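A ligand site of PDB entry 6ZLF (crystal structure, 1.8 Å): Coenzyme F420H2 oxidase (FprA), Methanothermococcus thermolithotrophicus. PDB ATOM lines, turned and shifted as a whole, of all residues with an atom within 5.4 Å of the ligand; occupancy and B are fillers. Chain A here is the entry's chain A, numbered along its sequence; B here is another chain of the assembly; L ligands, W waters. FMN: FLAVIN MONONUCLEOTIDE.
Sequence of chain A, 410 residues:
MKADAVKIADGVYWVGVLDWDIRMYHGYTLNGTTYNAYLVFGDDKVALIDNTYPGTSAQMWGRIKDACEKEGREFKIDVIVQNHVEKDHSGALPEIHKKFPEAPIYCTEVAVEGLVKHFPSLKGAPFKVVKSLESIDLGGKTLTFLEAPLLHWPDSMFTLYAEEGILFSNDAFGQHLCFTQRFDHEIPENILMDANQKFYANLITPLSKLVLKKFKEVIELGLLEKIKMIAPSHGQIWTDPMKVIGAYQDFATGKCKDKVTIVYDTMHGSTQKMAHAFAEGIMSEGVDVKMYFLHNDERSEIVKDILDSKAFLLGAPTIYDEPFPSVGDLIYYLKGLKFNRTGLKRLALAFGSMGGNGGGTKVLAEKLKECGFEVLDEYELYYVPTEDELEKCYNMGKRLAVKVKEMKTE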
ATOM      1  N   ASP A 265      21.455  18.848   4.672  1.00  0.00           N
ATOM      2  CA  ASP A 265      20.125  19.355   4.984  1.00  0.00           C
ATOM      3  C   ASP A 265      19.112  18.512   4.220  1.00  0.00           C
ATOM      4  O   ASP A 265      19.488  17.724   3.354  1.00  0.00           O
ATOM      5  CB  ASP A 265      19.969  20.848   4.665  1.00  0.00           C
ATOM      6  CG  ASP A 265      19.021  21.566   5.626  1.00  0.00           C
ATOM      7  OD1 ASP A 265      18.164  20.893   6.227  1.00  0.00           O
ATOM      8  OD2 ASP A 265      19.174  22.794   5.806  1.00  0.00           O
ATOM      9  N   THR A 266      17.851  18.576   4.639  1.00  0.00           N
ATOM     10  CA  THR A 266      16.794  17.765   4.061  1.00  0.00           C
ATOM     11  C   THR A 266      15.469  18.486   4.276  1.00  0.00           C
ATOM     12  O   THR A 266      15.298  19.190   5.265  1.00  0.00           O
ATOM     13  CB  THR A 266      16.805  16.358   4.732  1.00  0.00           C
ATOM     14  OG1 THR A 266      16.049  15.459   3.937  1.00  0.00           O
ATOM     15  CG2 THR A 266      16.229  16.364   6.155  1.00  0.00           C
ATOM     16  N   MET A 267      14.515  18.233   3.389  1.00  0.00           N
ATOM     17  CA  MET A 267      13.134  18.688   3.562  1.00  0.00           C
ATOM     18  C   MET A 267      12.254  17.505   3.967  1.00  0.00           C
ATOM     19  O   MET A 267      11.537  17.580   4.957  1.00  0.00           O
ATOM     20  CB  MET A 267      12.610  19.305   2.264  1.00  0.00           C
ATOM     21  CG  MET A 267      13.397  20.526   1.838  1.00  0.00           C
ATOM     22  SD  MET A 267      12.764  21.280   0.333  1.00  0.00           S
ATOM     23  CE  MET A 267      13.359  20.084  -0.903  1.00  0.00           C
ATOM     24  N   HIS A 268      12.340  16.398   3.223  1.00  0.00           N
ATOM     25  CA  HIS A 268      11.499  15.217   3.418  1.00  0.00           C
ATOM     26  C   HIS A 268      12.258  13.980   3.954  1.00  0.00           C
ATOM     27  O   HIS A 268      11.667  12.897   4.003  1.00  0.00           O
ATOM     28  CB  HIS A 268      10.800  14.868   2.093  1.00  0.00           C
ATOM     29  CG  HIS A 268       9.797  15.902   1.669  1.00  0.00           C
ATOM     30  ND1 HIS A 268       8.794  16.317   2.515  1.00  0.00           N
ATOM     31  CD2 HIS A 268       9.661  16.549   0.483  1.00  0.00           C
ATOM     32  CE1 HIS A 268       8.074  17.182   1.846  1.00  0.00           C
ATOM     33  NE2 HIS A 268       8.569  17.367   0.614  1.00  0.00           N
ATOM     34  N   GLY A 269      13.509  14.144   4.374  1.00  0.00           N
ATOM     35  CA  GLY A 269      14.265  13.074   5.036  1.00  0.00           C
ATOM     36  C   GLY A 269      15.110  12.162   4.163  1.00  0.00           C
ATOM     37  O   GLY A 269      15.841  11.319   4.705  1.00  0.00           O
ATOM     38  N   SER A 270      15.038  12.273   2.831  1.00  0.00           N
ATOM     39  CA  SER A 270      15.781  11.330   1.976  1.00  0.00           C
ATOM     40  C   SER A 270      17.292  11.575   2.001  1.00  0.00           C
ATOM     41  O   SER A 270      18.060  10.617   2.119  1.00  0.00           O
ATOM     42  CB  SER A 270      15.241  11.370   0.545  1.00  0.00           C
ATOM     43  OG  SER A 270      13.922  10.837   0.532  1.00  0.00           O
ATOM     44  N   THR A 271      17.714  12.845   1.980  1.00  0.00           N
ATOM     45  CA  THR A 271      19.146  13.162   2.048  1.00  0.00           C
ATOM     46  C   THR A 271      19.686  12.759   3.436  1.00  0.00           C
ATOM     47  O   THR A 271      20.818  12.291   3.534  1.00  0.00           O
ATOM     48  CB  THR A 271      19.371  14.635   1.714  1.00  0.00           C
ATOM     49  OG1 THR A 271      18.861  14.903   0.390  1.00  0.00           O
ATOM     50  CG2 THR A 271      20.841  15.033   1.774  1.00  0.00           C
ATOM     51  N   GLN A 272      18.852  12.870   4.479  1.00  0.00           N
ATOM     52  CA  GLN A 272      19.219  12.412   5.824  1.00  0.00           C
ATOM     53  C   GLN A 272      19.489  10.911   5.844  1.00  0.00           C
ATOM     54  O   GLN A 272      20.471  10.473   6.422  1.00  0.00           O
ATOM     55  CB  GLN A 272      18.096  12.771   6.805  1.00  0.00           C
ATOM     56  CG  GLN A 272      18.309  12.269   8.236  1.00  0.00           C
ATOM     57  CD  GLN A 272      17.226  12.854   9.114  1.00  0.00           C
ATOM     58  OE1 GLN A 272      16.037  12.587   8.910  1.00  0.00           O
ATOM     59  NE2 GLN A 272      17.578  13.726  10.044  1.00  0.00           N
ATOM     60  N   PRO A 317      19.112  18.251  -0.810  1.00  0.00           N
ATOM     61  CA  PRO A 317      18.192  18.015  -1.932  1.00  0.00           C
ATOM     62  C   PRO A 317      18.249  19.168  -2.946  1.00  0.00           C
ATOM     63  O   PRO A 317      18.753  20.247  -2.635  1.00  0.00           O
ATOM     64  CB  PRO A 317      16.829  17.947  -1.246  1.00  0.00           C
ATOM     65  CG  PRO A 317      16.966  18.858  -0.081  1.00  0.00           C
ATOM     66  CD  PRO A 317      18.378  18.627   0.417  1.00  0.00           C
ATOM     67  N   THR A 318      17.653  18.954  -4.117  1.00  0.00           N
ATOM     68  CA  THR A 318      17.583  19.983  -5.171  1.00  0.00           C
ATOM     69  C   THR A 318      16.264  20.744  -5.023  1.00  0.00           C
ATOM     70  O   THR A 318      15.207  20.130  -4.924  1.00  0.00           O
ATOM     71  CB  THR A 318      17.724  19.347  -6.561  1.00  0.00           C
ATOM     72  OG1 THR A 318      19.016  18.734  -6.684  1.00  0.00           O
ATOM     73  CG2 THR A 318      17.529  20.366  -7.703  1.00  0.00           C
ATOM     74  N   ILE A 319      16.338  22.078  -5.099  1.00  0.00           N
ATOM     75  CA  ILE A 319      15.173  22.964  -5.073  1.00  0.00           C
ATOM     76  C   ILE A 319      15.359  24.034  -6.169  1.00  0.00           C
ATOM     77  O   ILE A 319      16.350  24.758  -6.153  1.00  0.00           O
ATOM     78  CB  ILE A 319      14.957  23.542  -3.644  1.00  0.00           C
ATOM     79  CG1 ILE A 319      13.812  24.590  -3.599  1.00  0.00           C
ATOM     80  CG2 ILE A 319      16.242  24.118  -3.066  1.00  0.00           C
ATOM     81  CD1 ILE A 319      13.319  24.865  -2.161  1.00  0.00           C
ATOM     82  N   TYR A 320      14.492  24.018  -7.189  1.00  0.00           N
ATOM     83  CA  TYR A 320      14.628  24.922  -8.352  1.00  0.00           C
ATOM     84  C   TYR A 320      16.006  24.847  -9.005  1.00  0.00           C
ATOM     85  O   TYR A 320      16.639  25.887  -9.194  1.00  0.00           O
ATOM     86  CB  TYR A 320      14.322  26.375  -7.963  1.00  0.00           C
ATOM     87  CG  TYR A 320      13.068  26.536  -7.154  1.00  0.00           C
ATOM     88  CD1 TYR A 320      11.864  25.999  -7.595  1.00  0.00           C
ATOM     89  CD2 TYR A 320      13.073  27.195  -5.935  1.00  0.00           C
ATOM     90  CE1 TYR A 320      10.694  26.142  -6.855  1.00  0.00           C
ATOM     91  CE2 TYR A 320      11.928  27.284  -5.154  1.00  0.00           C
ATOM     92  CZ  TYR A 320      10.731  26.776  -5.629  1.00  0.00           C
ATOM     93  OH  TYR A 320       9.603  26.850  -4.848  1.00  0.00           O
ATOM     94  N   ASP A 321      16.499  23.623  -9.279  1.00  0.00           N
ATOM     95  CA  ASP A 321      17.791  23.360  -9.923  1.00  0.00           C
ATOM     96  C   ASP A 321      19.014  23.682  -9.048  1.00  0.00           C
ATOM     97  O   ASP A 321      20.147  23.540  -9.528  1.00  0.00           O
ATOM     98  CB  ASP A 321      17.917  24.113 -11.273  1.00  0.00           C
ATOM     99  CG  ASP A 321      16.728  23.935 -12.203  1.00  0.00           C
ATOM    100  OD1 ASP A 321      16.230  22.791 -12.316  1.00  0.00           O
ATOM    101  OD2 ASP A 321      16.300  24.926 -12.813  1.00  0.00           O
ATOM    102  N   SER A 353      19.168  13.939  -2.679  1.00  0.00           N
ATOM    103  CA  SER A 353      17.991  13.384  -3.329  1.00  0.00           C
ATOM    104  C   SER A 353      17.377  14.476  -4.211  1.00  0.00           C
ATOM    105  O   SER A 353      17.618  15.654  -3.988  1.00  0.00           O
ATOM    106  CB  SER A 353      17.003  12.889  -2.268  1.00  0.00           C
ATOM    107  OG  SER A 353      15.817  12.410  -2.863  1.00  0.00           O
ATOM    108  N   MET A 354      16.601  14.076  -5.228  1.00  0.00           N
ATOM    109  CA  MET A 354      15.976  15.044  -6.131  1.00  0.00           C
ATOM    110  C   MET A 354      14.687  14.410  -6.666  1.00  0.00           C
ATOM    111  O   MET A 354      14.426  13.264  -6.366  1.00  0.00           O
ATOM    112  CB  MET A 354      16.919  15.471  -7.281  1.00  0.00           C
ATOM    113  CG  MET A 354      17.566  14.335  -8.035  1.00  0.00           C
ATOM    114  SD  MET A 354      16.510  13.608  -9.299  1.00  0.00           S
ATOM    115  CE  MET A 354      17.666  12.511 -10.079  1.00  0.00           C
ATOM    116  N   GLY A 355      13.865  15.191  -7.353  1.00  0.00           N
ATOM    117  CA  GLY A 355      12.580  14.693  -7.840  1.00  0.00           C
ATOM    118  C   GLY A 355      12.254  15.027  -9.289  1.00  0.00           C
ATOM    119  O   GLY A 355      11.115  14.832  -9.719  1.00  0.00           O
ATOM    120  N   GLY A 356      13.242  15.487 -10.051  1.00  0.00           N
ATOM    121  CA  GLY A 356      13.015  15.848 -11.441  1.00  0.00           C
ATOM    122  C   GLY A 356      14.310  15.857 -12.236  1.00  0.00           C
ATOM    123  O   GLY A 356      14.924  14.811 -12.423  1.00  0.00           O
ATOM    124  N   ASN A 357      14.751  17.044 -12.657  1.00  0.00           N
ATOM    125  CA  ASN A 357      15.987  17.168 -13.428  1.00  0.00           C
ATOM    126  C   ASN A 357      17.238  17.103 -12.551  1.00  0.00           C
ATOM    127  O   ASN A 357      18.316  16.835 -13.066  1.00  0.00           O
ATOM    128  CB  ASN A 357      16.001  18.441 -14.260  1.00  0.00           C
ATOM    129  CG  ASN A 357      15.002  18.449 -15.394  1.00  0.00           C
ATOM    130  OD1 ASN A 357      14.159  19.339 -15.490  1.00  0.00           O
ATOM    131  ND2 ASN A 357      15.073  17.482 -16.305  1.00  0.00           N
ATOM    132  N   GLY A 358      17.094  17.292 -11.241  1.00  0.00           N
ATOM    133  CA  GLY A 358      18.232  17.235 -10.326  1.00  0.00           C
ATOM    134  C   GLY A 358      19.213  18.365 -10.587  1.00  0.00           C
ATOM    135  O   GLY A 358      18.825  19.424 -11.070  1.00  0.00           O
ATOM    136  N   TYR A 382      16.705   9.532  -6.823  1.00  0.00           N
ATOM    137  CA  TYR A 382      15.328   9.985  -6.999  1.00  0.00           C
ATOM    138  C   TYR A 382      14.502   9.735  -5.724  1.00  0.00           C
ATOM    139  O   TYR A 382      14.347   8.590  -5.306  1.00  0.00           O
ATOM    140  CB  TYR A 382      14.740   9.212  -8.202  1.00  0.00           C
ATOM    141  CG  TYR A 382      13.363   9.653  -8.655  1.00  0.00           C
ATOM    142  CD1 TYR A 382      13.138  10.947  -9.092  1.00  0.00           C
ATOM    143  CD2 TYR A 382      12.353   8.713  -8.836  1.00  0.00           C
ATOM    144  CE1 TYR A 382      11.917  11.315  -9.645  1.00  0.00           C
ATOM    145  CE2 TYR A 382      11.126   9.081  -9.376  1.00  0.00           C
ATOM    146  CZ  TYR A 382      10.908  10.376  -9.800  1.00  0.00           C
ATOM    147  OH  TYR A 382       9.702  10.747 -10.329  1.00  0.00           O
ATOM    148  N   TYR A 383      13.964  10.803  -5.100  1.00  0.00           N
ATOM    149  CA  TYR A 383      13.111  10.704  -3.927  1.00  0.00           C
ATOM    150  C   TYR A 383      13.685   9.763  -2.835  1.00  0.00           C
ATOM    151  O   TYR A 383      14.814   9.979  -2.410  1.00  0.00           O
ATOM    152  CB  TYR A 383      11.672  10.315  -4.328  1.00  0.00           C
ATOM    153  CG  TYR A 383      10.996  11.351  -5.197  1.00  0.00           C
ATOM    154  CD1 TYR A 383      10.950  12.690  -4.809  1.00  0.00           C
ATOM    155  CD2 TYR A 383      10.283  10.976  -6.316  1.00  0.00           C
ATOM    156  CE1 TYR A 383      10.239  13.626  -5.543  1.00  0.00           C
ATOM    157  CE2 TYR A 383       9.543  11.902  -7.056  1.00  0.00           C
ATOM    158  CZ  TYR A 383       9.563  13.232  -6.684  1.00  0.00           C
ATOM    159  OH  TYR A 383       8.886  14.166  -7.439  1.00  0.00           O
ATOM    160  N   VAL A 384      12.880   8.798  -2.325  1.00  0.00           N
ATOM    161  CA  VAL A 384      13.256   8.022  -1.143  1.00  0.00           C
ATOM    162  C   VAL A 384      14.220   6.905  -1.545  1.00  0.00           C
ATOM    163  O   VAL A 384      13.884   6.095  -2.408  1.00  0.00           O
ATOM    164  CB  VAL A 384      12.000   7.475  -0.419  1.00  0.00           C
ATOM    165  CG1 VAL A 384      12.368   6.617   0.787  1.00  0.00           C
ATOM    166  CG2 VAL A 384      11.082   8.622   0.000  1.00  0.00           C
ATOM    167  N   HIS B  26      10.091  23.039   5.625  1.00  0.00           N
ATOM    168  CA  HIS B  26      11.131  23.133   4.577  1.00  0.00           C
ATOM    169  C   HIS B  26      11.802  24.515   4.561  1.00  0.00           C
ATOM    170  O   HIS B  26      12.083  25.045   3.484  1.00  0.00           O
ATOM    171  CB  HIS B  26      10.568  22.849   3.174  1.00  0.00           C
ATOM    172  CG  HIS B  26       9.702  21.640   3.077  1.00  0.00           C
ATOM    173  ND1 HIS B  26       9.711  20.654   4.046  1.00  0.00           N
ATOM    174  CD2 HIS B  26       8.858  21.272   2.082  1.00  0.00           C
ATOM    175  CE1 HIS B  26       8.856  19.736   3.620  1.00  0.00           C
ATOM    176  NE2 HIS B  26       8.323  20.069   2.447  1.00  0.00           N
ATOM    177  N   GLU B  86       4.014  14.996  -3.661  1.00  0.00           N
ATOM    178  CA  GLU B  86       4.718  15.465  -2.462  1.00  0.00           C
ATOM    179  C   GLU B  86       3.983  14.978  -1.193  1.00  0.00           C
ATOM    180  O   GLU B  86       2.747  14.919  -1.180  1.00  0.00           O
ATOM    181  CB  GLU B  86       4.866  16.992  -2.490  1.00  0.00           C
ATOM    182  CG  GLU B  86       5.852  17.522  -1.471  1.00  0.00           C
ATOM    183  CD  GLU B  86       6.217  18.990  -1.630  1.00  0.00           C
ATOM    184  OE1 GLU B  86       7.024  19.489  -0.822  1.00  0.00           O
ATOM    185  OE2 GLU B  86       5.687  19.632  -2.572  1.00  0.00           O
ATOM    186  N   HIS B 118       8.296   6.883  -3.337  1.00  0.00           N
ATOM    187  CA  HIS B 118       8.027   7.359  -1.972  1.00  0.00           C
ATOM    188  C   HIS B 118       7.501   6.239  -1.083  1.00  0.00           C
ATOM    189  O   HIS B 118       7.851   6.177   0.092  1.00  0.00           O
ATOM    190  CB  HIS B 118       6.995   8.503  -1.968  1.00  0.00           C
ATOM    191  CG  HIS B 118       7.576   9.854  -2.278  1.00  0.00           C
ATOM    192  ND1 HIS B 118       7.739  10.280  -3.571  1.00  0.00           N
ATOM    193  CD2 HIS B 118       7.949  10.844  -1.435  1.00  0.00           C
ATOM    194  CE1 HIS B 118       8.177  11.531  -3.490  1.00  0.00           C
ATOM    195  NE2 HIS B 118       8.377  11.893  -2.227  1.00  0.00           N
ATOM    196  N   HIS B 152       3.446  22.666  -8.974  1.00  0.00           N
ATOM    197  CA  HIS B 152       4.859  23.090  -8.949  1.00  0.00           C
ATOM    198  C   HIS B 152       5.882  21.961  -9.227  1.00  0.00           C
ATOM    199  O   HIS B 152       7.061  22.259  -9.383  1.00  0.00           O
ATOM    200  CB  HIS B 152       5.187  23.827  -7.634  1.00  0.00           C
ATOM    201  CG  HIS B 152       5.371  22.948  -6.435  1.00  0.00           C
ATOM    202  ND1 HIS B 152       6.538  22.967  -5.699  1.00  0.00           N
ATOM    203  CD2 HIS B 152       4.476  22.154  -5.795  1.00  0.00           C
ATOM    204  CE1 HIS B 152       6.346  22.156  -4.671  1.00  0.00           C
ATOM    205  NE2 HIS B 152       5.126  21.626  -4.706  1.00  0.00           N
ATOM    206  N   TRP B 153       5.431  20.690  -9.331  1.00  0.00           N
ATOM    207  CA  TRP B 153       6.319  19.553  -9.622  1.00  0.00           C
ATOM    208  C   TRP B 153       5.931  18.917 -10.978  1.00  0.00           C
ATOM    209  O   TRP B 153       4.830  19.170 -11.476  1.00  0.00           O
ATOM    210  CB  TRP B 153       6.224  18.497  -8.494  1.00  0.00           C
ATOM    211  CG  TRP B 153       7.060  18.764  -7.263  1.00  0.00           C
ATOM    212  CD1 TRP B 153       7.593  19.954  -6.883  1.00  0.00           C
ATOM    213  CD2 TRP B 153       7.373  17.824  -6.224  1.00  0.00           C
ATOM    214  NE1 TRP B 153       8.244  19.809  -5.679  1.00  0.00           N
ATOM    215  CE2 TRP B 153       8.068  18.533  -5.215  1.00  0.00           C
ATOM    216  CE3 TRP B 153       6.993  16.502  -5.961  1.00  0.00           C
ATOM    217  CZ2 TRP B 153       8.514  17.912  -4.045  1.00  0.00           C
ATOM    218  CZ3 TRP B 153       7.422  15.897  -4.790  1.00  0.00           C
ATOM    219  CH2 TRP B 153       8.228  16.590  -3.877  1.00  0.00           C
ATOM    220  N   LEU B 203       7.148  29.636  -3.560  1.00  0.00           N
ATOM    221  CA  LEU B 203       6.862  28.421  -4.332  1.00  0.00           C
ATOM    222  C   LEU B 203       6.600  28.641  -5.818  1.00  0.00           C
ATOM    223  O   LEU B 203       6.768  27.696  -6.591  1.00  0.00           O
ATOM    224  CB  LEU B 203       5.680  27.678  -3.684  1.00  0.00           C
ATOM    225  CG  LEU B 203       6.016  27.105  -2.305  1.00  0.00           C
ATOM    226  CD1 LEU B 203       4.750  26.798  -1.510  1.00  0.00           C
ATOM    227  CD2 LEU B 203       6.881  25.835  -2.424  1.00  0.00           C
HETATM  228  N1  FMN L   1      13.743  18.249  -7.598  1.00  0.00           N
HETATM  229  C2  FMN L   1      14.494  18.433  -8.715  1.00  0.00           C
HETATM  230  O2  FMN L   1      15.124  17.504  -9.238  1.00  0.00           O
HETATM  231  N3  FMN L   1      14.563  19.708  -9.297  1.00  0.00           N
HETATM  232  C4  FMN L   1      13.935  20.852  -8.834  1.00  0.00           C
HETATM  233  O4  FMN L   1      14.115  21.916  -9.402  1.00  0.00           O
HETATM  234  C4A FMN L   1      13.142  20.641  -7.636  1.00  0.00           C
HETATM  235  N5  FMN L   1      12.513  21.663  -7.108  1.00  0.00           N
HETATM  236  C5A FMN L   1      11.832  21.468  -5.916  1.00  0.00           C
HETATM  237  C6  FMN L   1      11.226  22.560  -5.302  1.00  0.00           C
HETATM  238  C7  FMN L   1      10.594  22.443  -4.065  1.00  0.00           C
HETATM  239  C7M FMN L   1       9.983  23.675  -3.430  1.00  0.00           C
HETATM  240  C8  FMN L   1      10.559  21.192  -3.425  1.00  0.00           C
HETATM  241  C8M FMN L   1       9.913  21.011  -2.080  1.00  0.00           C
HETATM  242  C9  FMN L   1      11.144  20.096  -4.050  1.00  0.00           C
HETATM  243  C9A FMN L   1      11.776  20.213  -5.287  1.00  0.00           C
HETATM  244  N10 FMN L   1      12.395  19.122  -5.927  1.00  0.00           N
HETATM  245  C10 FMN L   1      13.109  19.300  -7.079  1.00  0.00           C
HETATM  246  C1' FMN L   1      12.170  17.752  -5.421  1.00  0.00           C
HETATM  247  C2' FMN L   1      13.099  17.401  -4.262  1.00  0.00           C
HETATM  248  O2' FMN L   1      14.469  17.523  -4.663  1.00  0.00           O
HETATM  249  C3' FMN L   1      12.817  15.957  -3.828  1.00  0.00           C
HETATM  250  O3' FMN L   1      11.562  15.975  -3.163  1.00  0.00           O
HETATM  251  C4' FMN L   1      13.877  15.346  -2.917  1.00  0.00           C
HETATM  252  O4' FMN L   1      13.652  13.938  -2.795  1.00  0.00           O
HETATM  253  C5' FMN L   1      13.902  15.976  -1.539  1.00  0.00           C
HETATM  254  O5' FMN L   1      14.933  15.310  -0.788  1.00  0.00           O
HETATM  255  P   FMN L   1      14.892  15.340   0.820  1.00  0.00           P
HETATM  256  O1P FMN L   1      16.281  15.123   1.307  1.00  0.00           O
HETATM  257  O2P FMN L   1      13.912  14.285   1.300  1.00  0.00           O
HETATM  258  O3P FMN L   1      14.316  16.729   1.179  1.00  0.00           O
HETATM  259  O   HOH W   1      11.130  19.008  -9.987  1.00  0.00           O
HETATM  260  O   HOH W   2      10.007  17.153  -8.049  1.00  0.00           O
HETATM  261  O   HOH W   3      10.398  14.072  -1.589  1.00  0.00           O
HETATM  262  O   HOH W   4      16.329  20.300 -11.347  1.00  0.00           O
HETATM  263  O   HOH W   5      12.573  12.885  -0.539  1.00  0.00           O
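An oxygen (O2) of the ligand is in hydrogen-bond range of the backbone NH of Asn 357 (3.5 Å). The backbone NH (N) of Asp 321 is in hydrogen-bond range of an oxygen (O4) of the ligand. N of Gly 269 is in hydrogen-bond range of O2P of the ligand. The backbone NH (N) of Tyr 320 is in hydrogen-bond range of an oxygen (O4) of the ligand, at 3.1 Å. An oxygen (O2') of the ligand is in hydrogen-bond range of the backbone carbonyl oxygen (O) of Thr 318 (2.7 Å). The backbone NH of Gly 355 sits at hydrogen-bond distance from a nitrogen (N1) of the ligand (3.1 Å). The backbone NH (N) of Gly 358 lies within hydrogen-bond range of an oxygen (O2) of the ligand. OG1 of Thr 266 lies within hydrogen-bond range of O1P of the ligand, at 2.7 Å. An oxygen (O1P) of the ligand lies within hydrogen-bond range of the backbone NH of Thr 271 (2.8 Å). N of His 268 is in hydrogen-bond range of O3P of the ligand, 2.9 Å away. N of Ser 270 sits at hydrogen-bond distance from O2P of the ligand (2.8 Å). The side-chain hydroxyl (OG1) of Thr 271 sits at hydrogen-bond distance from an oxygen (O1P) of the ligand (2.7 Å). The backbone NH (N) of Met 267 sits at hydrogen-bond distance from an oxygen (O3P) of the ligand, 2.7 Å away. An oxygen (O2) of the ligand is in hydrogen-bond range of the backbone NH of Gly 356, 2.9 Å away. O4' of the ligand is in hydrogen-bond range of OG of Ser 353 (2.7 Å).
The side-chain hydroxyl of Tyr 320 sits close to the backbone carbonyl oxygen of Leu 203 of chain B, 3.4 Å away. OG1 of Thr 266 sits at hydrogen-bond distance from N of Gly 269 (2.9 Å). N of Tyr 383 lies within hydrogen-bond range of O of Met 354 (2.8 Å). The side-chain hydroxyl (OH) of Tyr 383 lies within hydrogen-bond range of the backbone carbonyl oxygen (O) of Gly 355 (3.3 Å). The side-chain hydroxyl (OG) of Ser 270 sits at hydrogen-bond distance from the backbone carbonyl oxygen (O) of Tyr 383. O of Ser 353 is in hydrogen-bond range of N of Thr 318, at 3.3 Å. A ring nitrogen (NE2) of His 268 sits close to a ring nitrogen (NE2) of His 26 of chain B (3.3 Å). A ring nitrogen (NE2) of His 268 sits at hydrogen-bond distance from the side-chain carboxylate (OE1) of Glu 86 of chain B, 3.0 Å away.
CB of Pro 317 touches O5' of the ligand, 3.3 Å away. Ile 319 touches the ligand (CA to N5, 3.6 Å). Met 354 touches the ligand (CA to O2', 3.3 Å). Tyr 383 touches the ligand (CA to O4', 3.5 Å). Glu 86 of chain B touches the ligand. Trp 153 of chain B touches the ligand. CD2 of Leu 203 of chain B touches C7M of the ligand, 3.9 Å away. Hydrophobic or aromatic side chains that line the ligand: Met 267, His 268, Pro 317, Ile 319, Tyr 320, Met 354, Tyr 383, Trp 153 of chain B and Leu 203 of chain B. The nearest printed residue that does not touch the ligand is His 152 of chain B (4.1 Å).
Water W5 bridges an oxygen (O2P) of the ligand (2.7 Å) and the side-chain hydroxyl of Ser 270 (2.7 Å). Water W3 bridges an oxygen (O3') of the ligand (2.7 Å) and a ring nitrogen (NE2) of His 118 of chain B (3.0 Å). Water W4 lies within hydrogen-bond range of O of Gly 358, OD1 of Asp 321 and N3 of the ligand. Water W2 lies within hydrogen-bond range of the backbone carbonyl oxygen (O) of Gly 355 and the side-chain hydroxyl (OH) of Tyr 383.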
